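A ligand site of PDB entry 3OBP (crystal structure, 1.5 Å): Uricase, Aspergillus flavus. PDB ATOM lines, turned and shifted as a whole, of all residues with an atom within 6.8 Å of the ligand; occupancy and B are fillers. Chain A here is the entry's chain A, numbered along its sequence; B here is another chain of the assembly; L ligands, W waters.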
ATOM      1  N   SER A 158     -22.855 -27.164  17.642  1.00  0.00           N
ATOM      2  CA  SER A 158     -23.208 -27.336  16.259  1.00  0.00           C
ATOM      3  C   SER A 158     -22.009 -26.981  15.397  1.00  0.00           C
ATOM      4  O   SER A 158     -21.350 -25.961  15.552  1.00  0.00           O
ATOM      5  CB  SER A 158     -24.419 -26.490  15.859  1.00  0.00           C
ATOM      6  OG  SER A 158     -24.683 -26.503  14.484  1.00  0.00           O
ATOM      7  N   GLN A 159     -21.708 -27.869  14.459  1.00  0.00           N
ATOM      8  CA  GLN A 159     -20.607 -27.741  13.546  1.00  0.00           C
ATOM      9  C   GLN A 159     -21.026 -27.896  12.097  1.00  0.00           C
ATOM     10  O   GLN A 159     -22.086 -28.516  11.827  1.00  0.00           O
ATOM     11  CB  GLN A 159     -19.560 -28.826  13.907  1.00  0.00           C
ATOM     12  CG  GLN A 159     -19.213 -28.836  15.386  1.00  0.00           C
ATOM     13  CD  GLN A 159     -18.078 -29.807  15.711  1.00  0.00           C
ATOM     14  OE1 GLN A 159     -17.323 -30.186  14.824  1.00  0.00           O
ATOM     15  NE2 GLN A 159     -17.989 -30.178  16.979  1.00  0.00           N
ATOM     16  N   PHE A 160     -20.276 -27.401  11.143  1.00  0.00           N
ATOM     17  CA  PHE A 160     -20.504 -27.712   9.763  1.00  0.00           C
ATOM     18  C   PHE A 160     -19.223 -27.498   8.949  1.00  0.00           C
ATOM     19  O   PHE A 160     -18.870 -26.418   8.538  1.00  0.00           O
ATOM     20  CB  PHE A 160     -21.665 -26.911   9.146  1.00  0.00           C
ATOM     21  CG  PHE A 160     -22.114 -27.410   7.800  1.00  0.00           C
ATOM     22  CD1 PHE A 160     -22.598 -28.730   7.730  1.00  0.00           C
ATOM     23  CD2 PHE A 160     -22.062 -26.711   6.632  1.00  0.00           C
ATOM     24  CE1 PHE A 160     -22.969 -29.204   6.501  1.00  0.00           C
ATOM     25  CE2 PHE A 160     -22.450 -27.156   5.388  1.00  0.00           C
ATOM     26  CZ  PHE A 160     -22.919 -28.469   5.351  1.00  0.00           C
ATOM     27  N   PHE A 163     -17.720 -30.253   3.887  1.00  0.00           N
ATOM     28  CA  PHE A 163     -18.587 -30.271   2.754  1.00  0.00           C
ATOM     29  C   PHE A 163     -17.844 -30.020   1.434  1.00  0.00           C
ATOM     30  O   PHE A 163     -16.691 -29.569   1.495  1.00  0.00           O
ATOM     31  CB  PHE A 163     -19.727 -29.245   2.856  1.00  0.00           C
ATOM     32  CG  PHE A 163     -19.282 -27.844   3.294  1.00  0.00           C
ATOM     33  CD1 PHE A 163     -19.216 -27.490   4.611  1.00  0.00           C
ATOM     34  CD2 PHE A 163     -18.965 -26.941   2.294  1.00  0.00           C
ATOM     35  CE1 PHE A 163     -18.800 -26.196   4.970  1.00  0.00           C
ATOM     36  CE2 PHE A 163     -18.540 -25.651   2.639  1.00  0.00           C
ATOM     37  CZ  PHE A 163     -18.469 -25.314   3.968  1.00  0.00           C
ATOM     38  N   LEU A 171     -18.825 -20.423   1.375  1.00  0.00           N
ATOM     39  CA  LEU A 171     -19.049 -20.693   2.759  1.00  0.00           C
ATOM     40  C   LEU A 171     -17.796 -21.182   3.481  1.00  0.00           C
ATOM     41  O   LEU A 171     -17.159 -22.148   3.034  1.00  0.00           O
ATOM     42  CB  LEU A 171     -20.191 -21.741   2.930  1.00  0.00           C
ATOM     43  CG  LEU A 171     -20.527 -22.084   4.376  1.00  0.00           C
ATOM     44  CD1 LEU A 171     -21.240 -20.928   5.082  1.00  0.00           C
ATOM     45  CD2 LEU A 171     -21.382 -23.327   4.483  1.00  0.00           C
ATOM     46  N   ARG A 177     -21.134 -23.073  15.787  1.00  0.00           N
ATOM     47  CA  ARG A 177     -22.154 -22.164  15.244  1.00  0.00           C
ATOM     48  C   ARG A 177     -23.439 -22.347  16.062  1.00  0.00           C
ATOM     49  O   ARG A 177     -23.619 -23.240  16.861  1.00  0.00           O
ATOM     50  CB  ARG A 177     -22.431 -22.392  13.780  1.00  0.00           C
ATOM     51  CG  ARG A 177     -23.008 -23.778  13.473  1.00  0.00           C
ATOM     52  CD  ARG A 177     -23.330 -23.985  12.008  1.00  0.00           C
ATOM     53  NE  ARG A 177     -24.110 -25.251  11.879  1.00  0.00           N
ATOM     54  CZ  ARG A 177     -24.638 -25.669  10.740  1.00  0.00           C
ATOM     55  NH1 ARG A 177     -24.507 -25.030   9.615  1.00  0.00           N
ATOM     56  NH2 ARG A 177     -25.333 -26.827  10.722  1.00  0.00           N
ATOM     57  N   LEU A 179     -27.438 -23.095  16.033  1.00  0.00           N
ATOM     58  CA  LEU A 179     -28.407 -23.870  15.278  1.00  0.00           C
ATOM     59  C   LEU A 179     -29.829 -23.615  15.830  1.00  0.00           C
ATOM     60  O   LEU A 179     -30.107 -23.838  16.955  1.00  0.00           O
ATOM     61  CB  LEU A 179     -28.092 -25.364  15.330  1.00  0.00           C
ATOM     62  CG  LEU A 179     -28.984 -26.344  14.594  1.00  0.00           C
ATOM     63  CD1 LEU A 179     -29.099 -25.967  13.130  1.00  0.00           C
ATOM     64  CD2 LEU A 179     -28.486 -27.784  14.740  1.00  0.00           C
ATOM     65  N   SER A 225     -23.730 -31.537  17.017  1.00  0.00           N
ATOM     66  CA  SER A 225     -24.242 -31.806  15.695  1.00  0.00           C
ATOM     67  C   SER A 225     -23.231 -31.610  14.565  1.00  0.00           C
ATOM     68  O   SER A 225     -22.653 -30.537  14.424  1.00  0.00           O
ATOM     69  CB  SER A 225     -25.456 -30.894  15.453  1.00  0.00           C
ATOM     70  OG  SER A 225     -25.914 -30.915  14.135  1.00  0.00           O
ATOM     71  N   ALA A 226     -23.082 -32.608  13.714  1.00  0.00           N
ATOM     72  CA  ALA A 226     -22.227 -32.571  12.547  1.00  0.00           C
ATOM     73  C   ALA A 226     -22.847 -31.871  11.356  1.00  0.00           C
ATOM     74  O   ALA A 226     -22.218 -31.373  10.423  1.00  0.00           O
ATOM     75  CB  ALA A 226     -21.852 -34.026  12.216  1.00  0.00           C
ATOM     76  N   SER A 227     -24.181 -31.789  11.325  1.00  0.00           N
ATOM     77  CA  SER A 227     -25.033 -31.208  10.340  1.00  0.00           C
ATOM     78  C   SER A 227     -26.501 -31.440  10.783  1.00  0.00           C
ATOM     79  O   SER A 227     -26.736 -32.189  11.689  1.00  0.00           O
ATOM     80  CB  SER A 227     -24.849 -31.713   8.911  1.00  0.00           C
ATOM     81  OG  SER A 227     -25.230 -33.052   8.827  1.00  0.00           O
ATOM     82  N   VAL A 228     -27.368 -30.732  10.058  1.00  0.00           N
ATOM     83  CA  VAL A 228     -28.796 -30.929  10.348  1.00  0.00           C
ATOM     84  C   VAL A 228     -29.188 -32.354   9.896  1.00  0.00           C
ATOM     85  O   VAL A 228     -29.944 -32.970  10.645  1.00  0.00           O
ATOM     86  CB  VAL A 228     -29.676 -29.889   9.673  1.00  0.00           C
ATOM     87  CG1 VAL A 228     -31.156 -30.157   9.897  1.00  0.00           C
ATOM     88  CG2 VAL A 228     -29.364 -28.496  10.222  1.00  0.00           C
ATOM     89  N   GLN A 229     -28.689 -32.716   8.740  1.00  0.00           N
ATOM     90  CA  GLN A 229     -28.901 -34.094   8.242  1.00  0.00           C
ATOM     91  C   GLN A 229     -28.621 -35.180   9.264  1.00  0.00           C
ATOM     92  O   GLN A 229     -29.412 -36.097   9.557  1.00  0.00           O
ATOM     93  CB  GLN A 229     -27.988 -34.279   7.033  1.00  0.00           C
ATOM     94  CG  GLN A 229     -28.347 -33.543   5.782  1.00  0.00           C
ATOM     95  CD  GLN A 229     -27.846 -32.093   5.660  1.00  0.00           C
ATOM     96  OE1 GLN A 229     -27.508 -31.464   6.665  1.00  0.00           O
ATOM     97  NE2 GLN A 229     -27.818 -31.650   4.420  1.00  0.00           N
ATOM     98  N   ASN A 255     -33.063 -24.536   8.346  1.00  0.00           N
ATOM     99  CA  ASN A 255     -31.885 -24.014   9.074  1.00  0.00           C
ATOM    100  C   ASN A 255     -32.003 -22.480   9.013  1.00  0.00           C
ATOM    101  O   ASN A 255     -31.828 -21.938   7.932  1.00  0.00           O
ATOM    102  CB  ASN A 255     -30.618 -24.569   8.427  1.00  0.00           C
ATOM    103  CG  ASN A 255     -29.383 -24.278   9.268  1.00  0.00           C
ATOM    104  OD1 ASN A 255     -29.453 -23.645  10.298  1.00  0.00           O
ATOM    105  ND2 ASN A 255     -28.226 -24.792   8.794  1.00  0.00           N
ATOM    106  N   HIS A 257     -30.745 -19.252   9.740  1.00  0.00           N
ATOM    107  CA  HIS A 257     -29.356 -18.798   9.915  1.00  0.00           C
ATOM    108  C   HIS A 257     -29.161 -17.570  10.823  1.00  0.00           C
ATOM    109  O   HIS A 257     -29.971 -16.640  10.669  1.00  0.00           O
ATOM    110  CB  HIS A 257     -28.733 -18.465   8.573  1.00  0.00           C
ATOM    111  CG  HIS A 257     -28.800 -19.577   7.563  1.00  0.00           C
ATOM    112  ND1 HIS A 257     -28.235 -20.813   7.802  1.00  0.00           N
ATOM    113  CD2 HIS A 257     -29.375 -19.590   6.347  1.00  0.00           C
ATOM    114  CE1 HIS A 257     -28.472 -21.525   6.709  1.00  0.00           C
ATOM    115  NE2 HIS A 257     -29.156 -20.852   5.830  1.00  0.00           N
ATOM    116  N   GLY A 287     -31.878 -22.653   4.831  1.00  0.00           N
ATOM    117  CA  GLY A 287     -31.714 -24.041   4.358  1.00  0.00           C
ATOM    118  C   GLY A 287     -33.016 -24.779   4.651  1.00  0.00           C
ATOM    119  O   GLY A 287     -33.762 -24.467   5.583  1.00  0.00           O
ATOM    120  N   ILE A 289     -34.043 -28.965   4.951  1.00  0.00           N
ATOM    121  CA  ILE A 289     -33.500 -30.333   5.007  1.00  0.00           C
ATOM    122  C   ILE A 289     -34.614 -31.305   5.344  1.00  0.00           C
ATOM    123  O   ILE A 289     -35.294 -31.129   6.354  1.00  0.00           O
ATOM    124  CB  ILE A 289     -32.402 -30.415   6.079  1.00  0.00           C
ATOM    125  CG1 ILE A 289     -31.418 -29.225   6.073  1.00  0.00           C
ATOM    126  CG2 ILE A 289     -31.641 -31.721   5.972  1.00  0.00           C
ATOM    127  CD1 ILE A 289     -30.821 -29.000   4.720  1.00  0.00           C
ATOM    128  N   TYR B   9     -32.758 -31.939   0.032  1.00  0.00           N
ATOM    129  CA  TYR B   9     -32.285 -30.835   0.890  1.00  0.00           C
ATOM    130  C   TYR B   9     -31.912 -29.721  -0.079  1.00  0.00           C
ATOM    131  O   TYR B   9     -31.639 -29.869  -1.268  1.00  0.00           O
ATOM    132  CB  TYR B   9     -31.127 -31.245   1.776  1.00  0.00           C
ATOM    133  CG  TYR B   9     -29.820 -31.127   1.023  1.00  0.00           C
ATOM    134  CD1 TYR B   9     -29.515 -32.078   0.053  1.00  0.00           C
ATOM    135  CD2 TYR B   9     -28.933 -30.090   1.264  1.00  0.00           C
ATOM    136  CE1 TYR B   9     -28.331 -31.988  -0.660  1.00  0.00           C
ATOM    137  CE2 TYR B   9     -27.770 -29.991   0.550  1.00  0.00           C
ATOM    138  CZ  TYR B   9     -27.473 -30.938  -0.404  1.00  0.00           C
ATOM    139  OH  TYR B   9     -26.310 -30.847  -1.123  1.00  0.00           O
ATOM    140  N   GLY B  10     -31.905 -28.465   0.435  1.00  0.00           N
ATOM    141  CA  GLY B  10     -31.583 -27.341  -0.403  1.00  0.00           C
ATOM    142  C   GLY B  10     -31.816 -25.979   0.292  1.00  0.00           C
ATOM    143  O   GLY B  10     -31.768 -25.912   1.485  1.00  0.00           O
ATOM    144  N   LYS B  11     -32.083 -25.009  -0.585  1.00  0.00           N
ATOM    145  CA  LYS B  11     -32.274 -23.630  -0.098  1.00  0.00           C
ATOM    146  C   LYS B  11     -33.690 -23.164  -0.482  1.00  0.00           C
ATOM    147  O   LYS B  11     -34.064 -23.273  -1.636  1.00  0.00           O
ATOM    148  CB  LYS B  11     -31.209 -22.687  -0.676  1.00  0.00           C
ATOM    149  CG  LYS B  11     -31.020 -21.428   0.169  1.00  0.00           C
ATOM    150  CD  LYS B  11     -30.340 -21.738   1.464  1.00  0.00           C
ATOM    151  CE  LYS B  11     -29.282 -20.808   1.987  1.00  0.00           C
ATOM    152  NZ  LYS B  11     -28.532 -21.424   3.117  1.00  0.00           N
ATOM    153  N   ASN B  52     -20.056 -35.347   5.448  1.00  0.00           N
ATOM    154  CA  ASN B  52     -20.436 -34.130   4.731  1.00  0.00           C
ATOM    155  C   ASN B  52     -19.807 -33.995   3.361  1.00  0.00           C
ATOM    156  O   ASN B  52     -20.107 -33.131   2.556  1.00  0.00           O
ATOM    157  CB  ASN B  52     -20.110 -32.885   5.580  1.00  0.00           C
ATOM    158  CG  ASN B  52     -21.046 -32.736   6.744  1.00  0.00           C
ATOM    159  OD1 ASN B  52     -22.141 -33.295   6.684  1.00  0.00           O
ATOM    160  ND2 ASN B  52     -20.648 -32.011   7.768  1.00  0.00           N
ATOM    161  N   ILE B  55     -22.176 -33.416   0.494  1.00  0.00           N
ATOM    162  CA  ILE B  55     -23.086 -32.267   0.494  1.00  0.00           C
ATOM    163  C   ILE B  55     -22.574 -31.078  -0.315  1.00  0.00           C
ATOM    164  O   ILE B  55     -21.510 -30.534   0.020  1.00  0.00           O
ATOM    165  CB  ILE B  55     -23.385 -31.808   1.931  1.00  0.00           C
ATOM    166  CG1 ILE B  55     -23.967 -32.873   2.863  1.00  0.00           C
ATOM    167  CG2 ILE B  55     -24.338 -30.602   1.855  1.00  0.00           C
ATOM    168  CD1 ILE B  55     -24.130 -32.420   4.308  1.00  0.00           C
ATOM    169  N   VAL B  56     -23.332 -30.704  -1.298  1.00  0.00           N
ATOM    170  CA  VAL B  56     -23.274 -29.419  -1.978  1.00  0.00           C
ATOM    171  C   VAL B  56     -23.929 -28.437  -0.984  1.00  0.00           C
ATOM    172  O   VAL B  56     -25.146 -28.560  -0.769  1.00  0.00           O
ATOM    173  CB  VAL B  56     -23.923 -29.410  -3.359  1.00  0.00           C
ATOM    174  CG1 VAL B  56     -23.856 -28.047  -4.039  1.00  0.00           C
ATOM    175  CG2 VAL B  56     -23.261 -30.469  -4.266  1.00  0.00           C
ATOM    176  N   ALA B  57     -23.190 -27.552  -0.324  1.00  0.00           N
ATOM    177  CA  ALA B  57     -23.749 -26.683   0.706  1.00  0.00           C
ATOM    178  C   ALA B  57     -24.904 -25.853   0.146  1.00  0.00           C
ATOM    179  O   ALA B  57     -24.960 -25.388  -0.970  1.00  0.00           O
ATOM    180  CB  ALA B  57     -22.698 -25.777   1.344  1.00  0.00           C
ATOM    181  N   THR B  58     -25.902 -25.703   1.077  1.00  0.00           N
ATOM    182  CA  THR B  58     -27.079 -24.955   0.609  1.00  0.00           C
ATOM    183  C   THR B  58     -26.723 -23.481   0.331  1.00  0.00           C
ATOM    184  O   THR B  58     -27.332 -22.891  -0.551  1.00  0.00           O
ATOM    185  CB  THR B  58     -28.278 -24.994   1.578  1.00  0.00           C
ATOM    186  OG1 THR B  58     -27.967 -24.289   2.785  1.00  0.00           O
ATOM    187  CG2 THR B  58     -28.629 -26.427   1.977  1.00  0.00           C
ATOM    188  N   ASP B  59     -25.703 -23.001   1.055  1.00  0.00           N
ATOM    189  CA  ASP B  59     -25.159 -21.683   0.711  1.00  0.00           C
ATOM    190  C   ASP B  59     -24.644 -21.607  -0.716  1.00  0.00           C
ATOM    191  O   ASP B  59     -24.772 -20.635  -1.444  1.00  0.00           O
ATOM    192  CB  ASP B  59     -24.010 -21.317   1.656  1.00  0.00           C
ATOM    193  CG  ASP B  59     -23.603 -19.868   1.523  1.00  0.00           C
ATOM    194  OD1 ASP B  59     -24.367 -19.035   2.062  1.00  0.00           O
ATOM    195  OD2 ASP B  59     -22.575 -19.522   0.905  1.00  0.00           O
ATOM    196  N   SER B  60     -23.988 -22.701  -1.172  1.00  0.00           N
ATOM    197  CA  SER B  60     -23.543 -22.735  -2.566  1.00  0.00           C
ATOM    198  C   SER B  60     -24.657 -22.824  -3.591  1.00  0.00           C
ATOM    199  O   SER B  60     -24.645 -22.349  -4.720  1.00  0.00           O
ATOM    200  CB  SER B  60     -22.547 -23.905  -2.735  1.00  0.00           C
ATOM    201  OG  SER B  60     -21.602 -23.893  -1.693  1.00  0.00           O
HETATM  202  N1  LIG L   1     -26.509 -28.627   6.346  1.00  0.00           N
HETATM  203  C1  LIG L   1     -26.302 -27.942   7.536  1.00  0.00           C
HETATM  204  C2  LIG L   1     -26.350 -28.226   5.052  1.00  0.00           C
HETATM  205  N2  LIG L   1     -25.787 -26.662   7.397  1.00  0.00           N
HETATM  206  O1  LIG L   1     -26.475 -28.447   8.543  1.00  0.00           O
HETATM  207  C3  LIG L   1     -25.659 -26.185   6.171  1.00  0.00           C
HETATM  208  C4  LIG L   1     -25.879 -26.858   4.978  1.00  0.00           C
HETATM  209  N3  LIG L   1     -25.289 -24.916   5.789  1.00  0.00           N
HETATM  210  O2  LIG L   1     -26.591 -28.945   4.105  1.00  0.00           O
HETATM  211  N4  LIG L   1     -25.588 -26.176   3.924  1.00  0.00           N
HETATM  212  C5  LIG L   1     -25.223 -24.887   4.397  1.00  0.00           C
HETATM  213  O3  LIG L   1     -24.867 -23.940   3.648  1.00  0.00           O
HETATM  214  O   HOH W   1     -24.569 -22.435   7.398  1.00  0.00           O
HETATM  215  O   HOH W   2     -28.674 -25.278   5.563  1.00  0.00           O
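O2 of the ligand lies within hydrogen-bond range of NE2 of Gln 229. O1 of the ligand is in hydrogen-bond range of N of Val 228 (2.9 Å). The side-chain amide nitrogen (ND2) of Asn 255 sits close to a nitrogen (N2) of the ligand, at 3.4 Å. The backbone NH (N) of Thr 58 of chain B sits at hydrogen-bond distance from an oxygen (O3) of the ligand, 3.3 Å away. The side-chain hydroxyl (OG1) of Thr 58 of chain B is in hydrogen-bond range of an oxygen (O3) of the ligand, at 3.2 Å. The guanidinium group (NH2) of Arg 177 sits at hydrogen-bond distance from an oxygen (O1) of the ligand. The backbone NH (N) of Asp 59 of chain B sits at hydrogen-bond distance from an oxygen (O3) of the ligand, 2.9 Å away.
NZ of Lys 11 of chain B is in hydrogen-bond range of OG1 of Thr 58 of chain B (2.9 Å). OG of Ser 225 is in hydrogen-bond range of O of Ser 227, at 2.9 Å. The side-chain hydroxyl (OG) of Ser 227 sits close to the backbone NH (N) of Gln 229 (3.5 Å). The backbone carbonyl oxygen (O) of Gly 287 lies within hydrogen-bond range of the backbone NH (N) of Asn 255, 2.9 Å away. The backbone NH (N) of Arg 177 is in hydrogen-bond range of the backbone carbonyl oxygen (O) of Ser 158, at 2.9 Å. O of Val 56 of chain B is in hydrogen-bond range of OH of Tyr 9 of chain B.
Phe 160 touches the ligand. Leu 171 touches the ligand (CD2 to O3, 3.6 Å). CA of Ser 227 touches O1 of the ligand (3.6 Å). CD2 of Tyr 9 of chain B touches O2 of the ligand (3.9 Å). CG2 of Ile 55 of chain B touches O2 of the ligand (3.6 Å). Ala 57 of chain B touches the ligand (CB to O3, 3.7 Å). Hydrophobic or aromatic side chains within 4 Å of the ligand: Phe 160, Leu 171, Val 228, Tyr 9 of chain B, Ile 55 of chain B and Ala 57 of chain B. 12 residues have an atom within 4 Å of the ligand: Phe 160, Leu 171, Arg 177, Ser 227, Val 228, Gln 229, Asn 255, Tyr 9 of chain B, Ile 55 of chain B, Ala 57 of chain B, Thr 58 of chain B and Asp 59 of chain B. The nearest printed residue that does not touch the ligand is Ile 289 (4.3 Å).
Water W1 bridges N3 of the ligand (3.0 Å) and NH1 of Arg 177 (3.4 Å). Water W2 lies within hydrogen-bond range of OG1 of Thr 58 of chain B, ND2 of Asn 255 and N3 of the ligand.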
